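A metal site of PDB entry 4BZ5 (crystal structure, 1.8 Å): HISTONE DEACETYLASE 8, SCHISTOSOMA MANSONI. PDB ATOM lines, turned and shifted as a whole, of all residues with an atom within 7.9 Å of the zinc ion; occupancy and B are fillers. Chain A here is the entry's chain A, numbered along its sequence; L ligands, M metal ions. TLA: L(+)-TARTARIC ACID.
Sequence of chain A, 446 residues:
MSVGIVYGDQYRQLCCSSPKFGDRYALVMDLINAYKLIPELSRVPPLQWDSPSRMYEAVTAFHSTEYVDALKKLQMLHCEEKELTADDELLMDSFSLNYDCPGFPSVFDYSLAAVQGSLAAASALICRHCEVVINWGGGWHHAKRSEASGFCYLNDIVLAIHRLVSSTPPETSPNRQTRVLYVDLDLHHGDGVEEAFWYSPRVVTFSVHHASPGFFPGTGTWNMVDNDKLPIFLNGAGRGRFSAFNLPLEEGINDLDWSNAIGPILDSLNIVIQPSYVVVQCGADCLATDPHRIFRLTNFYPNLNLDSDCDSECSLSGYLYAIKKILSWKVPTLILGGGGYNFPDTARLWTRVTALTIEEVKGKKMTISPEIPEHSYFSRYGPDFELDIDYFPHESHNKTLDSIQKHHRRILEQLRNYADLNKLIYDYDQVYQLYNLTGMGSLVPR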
ATOM      1  N   LYS A  20      16.287   7.381  -8.305  1.00  0.00           N
ATOM      2  CA  LYS A  20      15.339   6.617  -7.504  1.00  0.00           C
ATOM      3  C   LYS A  20      15.312   7.030  -6.027  1.00  0.00           C
ATOM      4  O   LYS A  20      14.237   7.185  -5.442  1.00  0.00           O
ATOM      5  CB  LYS A  20      15.584   5.114  -7.605  1.00  0.00           C
ATOM      6  CG  LYS A  20      14.600   4.301  -6.769  1.00  0.00           C
ATOM      7  CD  LYS A  20      14.988   2.825  -6.688  1.00  0.00           C
ATOM      8  CE  LYS A  20      13.929   2.033  -5.926  1.00  0.00           C
ATOM      9  NZ  LYS A  20      14.411   0.653  -5.584  1.00  0.00           N
ATOM     10  N   PHE A  21      16.477   7.202  -5.430  1.00  0.00           N
ATOM     11  CA  PHE A  21      16.515   7.457  -3.985  1.00  0.00           C
ATOM     12  C   PHE A  21      16.675   8.930  -3.630  1.00  0.00           C
ATOM     13  O   PHE A  21      16.579   9.304  -2.467  1.00  0.00           O
ATOM     14  CB  PHE A  21      17.563   6.570  -3.288  1.00  0.00           C
ATOM     15  CG  PHE A  21      17.148   5.131  -3.232  1.00  0.00           C
ATOM     16  CD1 PHE A  21      16.113   4.728  -2.409  1.00  0.00           C
ATOM     17  CD2 PHE A  21      17.776   4.185  -4.023  1.00  0.00           C
ATOM     18  CE1 PHE A  21      15.728   3.398  -2.365  1.00  0.00           C
ATOM     19  CE2 PHE A  21      17.388   2.861  -3.986  1.00  0.00           C
ATOM     20  CZ  PHE A  21      16.354   2.468  -3.152  1.00  0.00           C
ATOM     21  N   GLY A 139      23.881  -1.159   1.380  1.00  0.00           N
ATOM     22  CA  GLY A 139      22.918  -2.237   1.534  1.00  0.00           C
ATOM     23  C   GLY A 139      22.355  -2.749   0.205  1.00  0.00           C
ATOM     24  O   GLY A 139      21.238  -3.254   0.148  1.00  0.00           O
ATOM     25  N   TRP A 140      23.152  -2.647  -0.857  1.00  0.00           N
ATOM     26  CA  TRP A 140      22.636  -2.898  -2.201  1.00  0.00           C
ATOM     27  C   TRP A 140      22.724  -4.364  -2.624  1.00  0.00           C
ATOM     28  O   TRP A 140      23.527  -4.775  -3.478  1.00  0.00           O
ATOM     29  CB  TRP A 140      23.236  -1.899  -3.184  1.00  0.00           C
ATOM     30  CG  TRP A 140      23.025  -0.500  -2.652  1.00  0.00           C
ATOM     31  CD1 TRP A 140      23.980   0.394  -2.265  1.00  0.00           C
ATOM     32  CD2 TRP A 140      21.755   0.132  -2.390  1.00  0.00           C
ATOM     33  NE1 TRP A 140      23.392   1.551  -1.793  1.00  0.00           N
ATOM     34  CE2 TRP A 140      22.029   1.412  -1.858  1.00  0.00           C
ATOM     35  CE3 TRP A 140      20.419  -0.261  -2.552  1.00  0.00           C
ATOM     36  CZ2 TRP A 140      21.016   2.314  -1.492  1.00  0.00           C
ATOM     37  CZ3 TRP A 140      19.419   0.633  -2.198  1.00  0.00           C
ATOM     38  CH2 TRP A 140      19.723   1.902  -1.675  1.00  0.00           C
ATOM     39  N   HIS A 141      21.842  -5.155  -2.018  1.00  0.00           N
ATOM     40  CA  HIS A 141      21.968  -6.601  -1.996  1.00  0.00           C
ATOM     41  C   HIS A 141      21.704  -7.352  -3.299  1.00  0.00           C
ATOM     42  O   HIS A 141      22.084  -8.510  -3.416  1.00  0.00           O
ATOM     43  CB  HIS A 141      21.114  -7.187  -0.854  1.00  0.00           C
ATOM     44  CG  HIS A 141      19.663  -6.798  -0.912  1.00  0.00           C
ATOM     45  ND1 HIS A 141      18.710  -7.419  -0.133  1.00  0.00           N
ATOM     46  CD2 HIS A 141      19.010  -5.857  -1.627  1.00  0.00           C
ATOM     47  CE1 HIS A 141      17.521  -6.874  -0.372  1.00  0.00           C
ATOM     48  NE2 HIS A 141      17.684  -5.920  -1.278  1.00  0.00           N
ATOM     49  N   HIS A 142      21.062  -6.704  -4.275  1.00  0.00           N
ATOM     50  CA  HIS A 142      20.694  -7.386  -5.524  1.00  0.00           C
ATOM     51  C   HIS A 142      21.781  -7.390  -6.612  1.00  0.00           C
ATOM     52  O   HIS A 142      21.667  -8.128  -7.581  1.00  0.00           O
ATOM     53  CB  HIS A 142      19.425  -6.778  -6.130  1.00  0.00           C
ATOM     54  CG  HIS A 142      18.227  -6.829  -5.237  1.00  0.00           C
ATOM     55  ND1 HIS A 142      17.738  -8.000  -4.708  1.00  0.00           N
ATOM     56  CD2 HIS A 142      17.401  -5.844  -4.797  1.00  0.00           C
ATOM     57  CE1 HIS A 142      16.673  -7.744  -3.967  1.00  0.00           C
ATOM     58  NE2 HIS A 142      16.445  -6.439  -4.003  1.00  0.00           N
ATOM     59  N   GLY A 150      17.551  -4.418  -9.587  1.00  0.00           N
ATOM     60  CA  GLY A 150      16.778  -3.734  -8.542  1.00  0.00           C
ATOM     61  C   GLY A 150      17.385  -2.441  -8.009  1.00  0.00           C
ATOM     62  O   GLY A 150      17.394  -2.200  -6.787  1.00  0.00           O
ATOM     63  N   CYS A 152      20.380  -1.791  -7.800  1.00  0.00           N
ATOM     64  CA  CYS A 152      21.659  -2.095  -7.180  1.00  0.00           C
ATOM     65  C   CYS A 152      22.703  -2.284  -8.273  1.00  0.00           C
ATOM     66  O   CYS A 152      22.566  -3.188  -9.113  1.00  0.00           O
ATOM     67  CB  CYS A 152      21.562  -3.364  -6.328  1.00  0.00           C
ATOM     68  SG  CYS A 152      20.325  -3.264  -5.001  1.00  0.00           S
ATOM     69  N   ASP A 184      19.452 -10.487   6.281  1.00  0.00           N
ATOM     70  CA  ASP A 184      18.854  -9.562   5.323  1.00  0.00           C
ATOM     71  C   ASP A 184      17.391  -9.371   5.715  1.00  0.00           C
ATOM     72  O   ASP A 184      16.588 -10.295   5.596  1.00  0.00           O
ATOM     73  CB  ASP A 184      19.007 -10.146   3.901  1.00  0.00           C
ATOM     74  CG  ASP A 184      18.717  -9.128   2.797  1.00  0.00           C
ATOM     75  OD1 ASP A 184      17.789  -8.329   2.970  1.00  0.00           O
ATOM     76  OD2 ASP A 184      19.396  -9.134   1.748  1.00  0.00           O
ATOM     77  N   LEU A 185      17.042  -8.180   6.217  1.00  0.00           N
ATOM     78  CA  LEU A 185      15.700  -7.906   6.722  1.00  0.00           C
ATOM     79  C   LEU A 185      14.791  -7.169   5.711  1.00  0.00           C
ATOM     80  O   LEU A 185      13.632  -6.889   6.017  1.00  0.00           O
ATOM     81  CB  LEU A 185      15.784  -7.086   8.015  1.00  0.00           C
ATOM     82  CG  LEU A 185      16.602  -7.669   9.156  1.00  0.00           C
ATOM     83  CD1 LEU A 185      16.561  -6.740  10.384  1.00  0.00           C
ATOM     84  CD2 LEU A 185      16.123  -9.043   9.543  1.00  0.00           C
ATOM     85  N   ASP A 186      15.335  -6.844   4.542  1.00  0.00           N
ATOM     86  CA  ASP A 186      14.623  -6.143   3.464  1.00  0.00           C
ATOM     87  C   ASP A 186      13.341  -6.887   3.055  1.00  0.00           C
ATOM     88  O   ASP A 186      13.180  -8.067   3.329  1.00  0.00           O
ATOM     89  CB  ASP A 186      15.595  -6.041   2.276  1.00  0.00           C
ATOM     90  CG  ASP A 186      15.145  -5.065   1.213  1.00  0.00           C
ATOM     91  OD1 ASP A 186      14.362  -5.460   0.333  1.00  0.00           O
ATOM     92  OD2 ASP A 186      15.628  -3.920   1.218  1.00  0.00           O
ATOM     93  N   LEU A 187      12.409  -6.208   2.407  1.00  0.00           N
ATOM     94  CA  LEU A 187      11.201  -6.878   1.913  1.00  0.00           C
ATOM     95  C   LEU A 187      11.551  -7.918   0.852  1.00  0.00           C
ATOM     96  O   LEU A 187      10.857  -8.934   0.681  1.00  0.00           O
ATOM     97  CB  LEU A 187      10.247  -5.830   1.335  1.00  0.00           C
ATOM     98  CG  LEU A 187       8.935  -6.319   0.711  1.00  0.00           C
ATOM     99  CD1 LEU A 187       8.011  -6.926   1.760  1.00  0.00           C
ATOM    100  CD2 LEU A 187       8.260  -5.155   0.007  1.00  0.00           C
ATOM    101  N   HIS A 188      12.645  -7.669   0.144  1.00  0.00           N
ATOM    102  CA  HIS A 188      13.007  -8.513  -0.996  1.00  0.00           C
ATOM    103  C   HIS A 188      14.116  -9.476  -0.658  1.00  0.00           C
ATOM    104  O   HIS A 188      15.000  -9.144   0.115  1.00  0.00           O
ATOM    105  CB  HIS A 188      13.459  -7.628  -2.148  1.00  0.00           C
ATOM    106  CG  HIS A 188      12.418  -6.663  -2.602  1.00  0.00           C
ATOM    107  ND1 HIS A 188      12.326  -5.375  -2.116  1.00  0.00           N
ATOM    108  CD2 HIS A 188      11.409  -6.804  -3.486  1.00  0.00           C
ATOM    109  CE1 HIS A 188      11.303  -4.764  -2.683  1.00  0.00           C
ATOM    110  NE2 HIS A 188      10.734  -5.608  -3.529  1.00  0.00           N
ATOM    111  N   HIS A 189      14.110 -10.661  -1.271  1.00  0.00           N
ATOM    112  CA  HIS A 189      15.157 -11.657  -1.073  1.00  0.00           C
ATOM    113  C   HIS A 189      16.556 -11.108  -1.363  1.00  0.00           C
ATOM    114  O   HIS A 189      16.785 -10.457  -2.389  1.00  0.00           O
ATOM    115  CB  HIS A 189      14.881 -12.854  -1.991  1.00  0.00           C
ATOM    116  CG  HIS A 189      15.941 -13.912  -1.946  1.00  0.00           C
ATOM    117  ND1 HIS A 189      16.519 -14.427  -3.070  1.00  0.00           N
ATOM    118  CD2 HIS A 189      16.522 -14.547  -0.886  1.00  0.00           C
ATOM    119  CE1 HIS A 189      17.410 -15.352  -2.734  1.00  0.00           C
ATOM    120  NE2 HIS A 189      17.433 -15.433  -1.415  1.00  0.00           N
ATOM    121  N   PHE A 215       6.676 -11.711  -8.059  1.00  0.00           N
ATOM    122  CA  PHE A 215       7.241 -10.705  -7.167  1.00  0.00           C
ATOM    123  C   PHE A 215       8.766 -10.762  -7.197  1.00  0.00           C
ATOM    124  O   PHE A 215       9.354 -11.839  -7.078  1.00  0.00           O
ATOM    125  CB  PHE A 215       6.738 -10.922  -5.735  1.00  0.00           C
ATOM    126  CG  PHE A 215       7.153  -9.849  -4.759  1.00  0.00           C
ATOM    127  CD1 PHE A 215       6.463  -8.647  -4.712  1.00  0.00           C
ATOM    128  CD2 PHE A 215       8.204 -10.060  -3.886  1.00  0.00           C
ATOM    129  CE1 PHE A 215       6.828  -7.661  -3.817  1.00  0.00           C
ATOM    130  CE2 PHE A 215       8.567  -9.057  -2.987  1.00  0.00           C
ATOM    131  CZ  PHE A 215       7.881  -7.861  -2.964  1.00  0.00           C
ATOM    132  N   PHE A 216       9.410  -9.601  -7.341  1.00  0.00           N
ATOM    133  CA  PHE A 216      10.867  -9.511  -7.490  1.00  0.00           C
ATOM    134  C   PHE A 216      11.622  -9.992  -6.240  1.00  0.00           C
ATOM    135  O   PHE A 216      11.224  -9.686  -5.123  1.00  0.00           O
ATOM    136  CB  PHE A 216      11.238  -8.053  -7.789  1.00  0.00           C
ATOM    137  CG  PHE A 216      12.707  -7.824  -7.986  1.00  0.00           C
ATOM    138  CD1 PHE A 216      13.315  -8.063  -9.213  1.00  0.00           C
ATOM    139  CD2 PHE A 216      13.477  -7.330  -6.957  1.00  0.00           C
ATOM    140  CE1 PHE A 216      14.666  -7.842  -9.392  1.00  0.00           C
ATOM    141  CE2 PHE A 216      14.834  -7.102  -7.131  1.00  0.00           C
ATOM    142  CZ  PHE A 216      15.426  -7.365  -8.347  1.00  0.00           C
ATOM    143  N   GLN A 281      21.420  -6.249   6.802  1.00  0.00           N
ATOM    144  CA  GLN A 281      20.822  -5.333   5.834  1.00  0.00           C
ATOM    145  C   GLN A 281      19.445  -4.969   6.392  1.00  0.00           C
ATOM    146  O   GLN A 281      18.633  -5.857   6.675  1.00  0.00           O
ATOM    147  CB  GLN A 281      20.745  -6.019   4.458  1.00  0.00           C
ATOM    148  CG  GLN A 281      20.520  -5.074   3.277  1.00  0.00           C
ATOM    149  CD  GLN A 281      19.060  -4.841   2.970  1.00  0.00           C
ATOM    150  OE1 GLN A 281      18.195  -5.064   3.810  1.00  0.00           O
ATOM    151  NE2 GLN A 281      18.781  -4.385   1.751  1.00  0.00           N
ATOM    152  N   GLY A 283      16.841  -2.966   5.071  1.00  0.00           N
ATOM    153  CA  GLY A 283      15.943  -2.321   4.122  1.00  0.00           C
ATOM    154  C   GLY A 283      14.606  -2.017   4.769  1.00  0.00           C
ATOM    155  O   GLY A 283      14.039  -2.876   5.448  1.00  0.00           O
ATOM    156  N   ALA A 284      14.095  -0.810   4.553  1.00  0.00           N
ATOM    157  CA  ALA A 284      12.943  -0.296   5.294  1.00  0.00           C
ATOM    158  C   ALA A 284      11.609  -0.517   4.593  1.00  0.00           C
ATOM    159  O   ALA A 284      10.579   0.066   4.978  1.00  0.00           O
ATOM    160  CB  ALA A 284      13.139   1.189   5.571  1.00  0.00           C
ATOM    161  N   ASP A 285      11.607  -1.354   3.548  1.00  0.00           N
ATOM    162  CA  ASP A 285      10.412  -1.551   2.747  1.00  0.00           C
ATOM    163  C   ASP A 285       9.390  -2.542   3.317  1.00  0.00           C
ATOM    164  O   ASP A 285       8.346  -2.797   2.706  1.00  0.00           O
ATOM    165  CB  ASP A 285      10.745  -1.873   1.278  1.00  0.00           C
ATOM    166  CG  ASP A 285      11.931  -2.805   1.124  1.00  0.00           C
ATOM    167  OD1 ASP A 285      12.422  -3.368   2.112  1.00  0.00           O
ATOM    168  OD2 ASP A 285      12.343  -2.979  -0.035  1.00  0.00           O
ATOM    169  N   CYS A 286       9.671  -3.079   4.504  1.00  0.00           N
ATOM    170  CA  CYS A 286       8.680  -3.888   5.223  1.00  0.00           C
ATOM    171  C   CYS A 286       7.694  -3.021   6.008  1.00  0.00           C
ATOM    172  O   CYS A 286       6.688  -3.537   6.505  1.00  0.00           O
ATOM    173  CB  CYS A 286       9.347  -4.866   6.189  1.00  0.00           C
ATOM    174  SG  CYS A 286      10.443  -6.074   5.411  1.00  0.00           S
ATOM    175  N   ASP A 290       5.154   1.627   3.561  1.00  0.00           N
ATOM    176  CA  ASP A 290       5.877   1.531   2.299  1.00  0.00           C
ATOM    177  C   ASP A 290       4.867   1.436   1.157  1.00  0.00           C
ATOM    178  O   ASP A 290       3.821   0.806   1.304  1.00  0.00           O
ATOM    179  CB  ASP A 290       6.791   0.303   2.299  1.00  0.00           C
ATOM    180  CG  ASP A 290       7.626   0.218   1.024  1.00  0.00           C
ATOM    181  OD1 ASP A 290       7.150  -0.380   0.034  1.00  0.00           O
ATOM    182  OD2 ASP A 290       8.750   0.765   1.034  1.00  0.00           O
ATOM    183  N   HIS A 292       4.839  -0.385  -1.357  1.00  0.00           N
ATOM    184  CA  HIS A 292       4.577  -1.758  -1.779  1.00  0.00           C
ATOM    185  C   HIS A 292       3.326  -2.277  -1.103  1.00  0.00           C
ATOM    186  O   HIS A 292       2.557  -3.050  -1.687  1.00  0.00           O
ATOM    187  CB  HIS A 292       5.746  -2.680  -1.432  1.00  0.00           C
ATOM    188  CG  HIS A 292       6.912  -2.554  -2.353  1.00  0.00           C
ATOM    189  ND1 HIS A 292       7.952  -1.681  -2.129  1.00  0.00           N
ATOM    190  CD2 HIS A 292       7.206  -3.197  -3.519  1.00  0.00           C
ATOM    191  CE1 HIS A 292       8.833  -1.776  -3.103  1.00  0.00           C
ATOM    192  NE2 HIS A 292       8.405  -2.695  -3.961  1.00  0.00           N
ATOM    193  N   GLY A 338      19.213  -0.092   2.662  1.00  0.00           N
ATOM    194  CA  GLY A 338      18.652  -0.909   1.594  1.00  0.00           C
ATOM    195  C   GLY A 338      17.393  -0.246   1.062  1.00  0.00           C
ATOM    196  O   GLY A 338      17.343   0.969   0.951  1.00  0.00           O
ATOM    197  N   GLY A 339      16.382  -1.048   0.736  1.00  0.00           N
ATOM    198  CA  GLY A 339      15.170  -0.521   0.126  1.00  0.00           C
ATOM    199  C   GLY A 339      14.376   0.405   1.033  1.00  0.00           C
ATOM    200  O   GLY A 339      14.684   0.556   2.215  1.00  0.00           O
ATOM    201  N   GLY A 340      13.344   1.027   0.467  1.00  0.00           N
ATOM    202  CA  GLY A 340      12.485   1.918   1.217  1.00  0.00           C
ATOM    203  C   GLY A 340      12.236   3.182   0.424  1.00  0.00           C
ATOM    204  O   GLY A 340      13.089   4.074   0.381  1.00  0.00           O
HETATM  205  O1  TLA L   1      15.641  -4.151  -2.026  1.00  0.00           O
HETATM  206  O11 TLA L   1      17.102  -2.908  -3.092  1.00  0.00           O
HETATM  207  C1  TLA L   1      15.924  -3.234  -2.815  1.00  0.00           C
HETATM  208  C2  TLA L   1      14.797  -2.497  -3.482  1.00  0.00           C
HETATM  209  O2  TLA L   1      13.659  -2.498  -2.616  1.00  0.00           O
HETATM  210  C3  TLA L   1      14.478  -3.192  -4.796  1.00  0.00           C
HETATM  211  O3  TLA L   1      14.378  -4.599  -4.568  1.00  0.00           O
HETATM  212  C4  TLA L   1      13.203  -2.700  -5.422  1.00  0.00           C
HETATM  213  O4  TLA L   1      13.066  -1.474  -5.644  1.00  0.00           O
HETATM  214  O41 TLA L   1      12.319  -3.543  -5.685  1.00  0.00           O
HETATM  215 ZN    ZN M   1      13.665  -4.164  -1.008  1.00  0.00          ZN
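The side-chain carboxylate (OD2) of Asp 186 is in hydrogen-bond range of the backbone NH (N) of Gly 339, 3.0 Å away.
The side-chain amide nitrogen (NE2) of Gln 281 sits at hydrogen-bond distance from the side-chain carboxylate (OD2) of Asp 186 (3.2 Å).
The side-chain carboxylate (OD1) of Asp 184 sits close to the backbone NH (N) of Asp 186 (3.3 Å).
The side-chain carboxylate (OD1) of Asp 285 is in hydrogen-bond range of the backbone NH (N) of Leu 187.
The nearest printed residue that does not touch the zinc ion is Gly 339 (4.1 Å).
The zinc ion is bound by the side-chain carboxylate (OD1) of Asp 186 (2.0 Å), the side-chain carboxylate (OD2) of Asp 285 (2.0 Å), a ring nitrogen (ND1) of His 188 (2.1 Å), an oxygen (O1) of the ligand (2.2 Å) and an oxygen (O2) of the ligand (2.3 Å).
The zinc ion has five donor atoms within binding distance.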
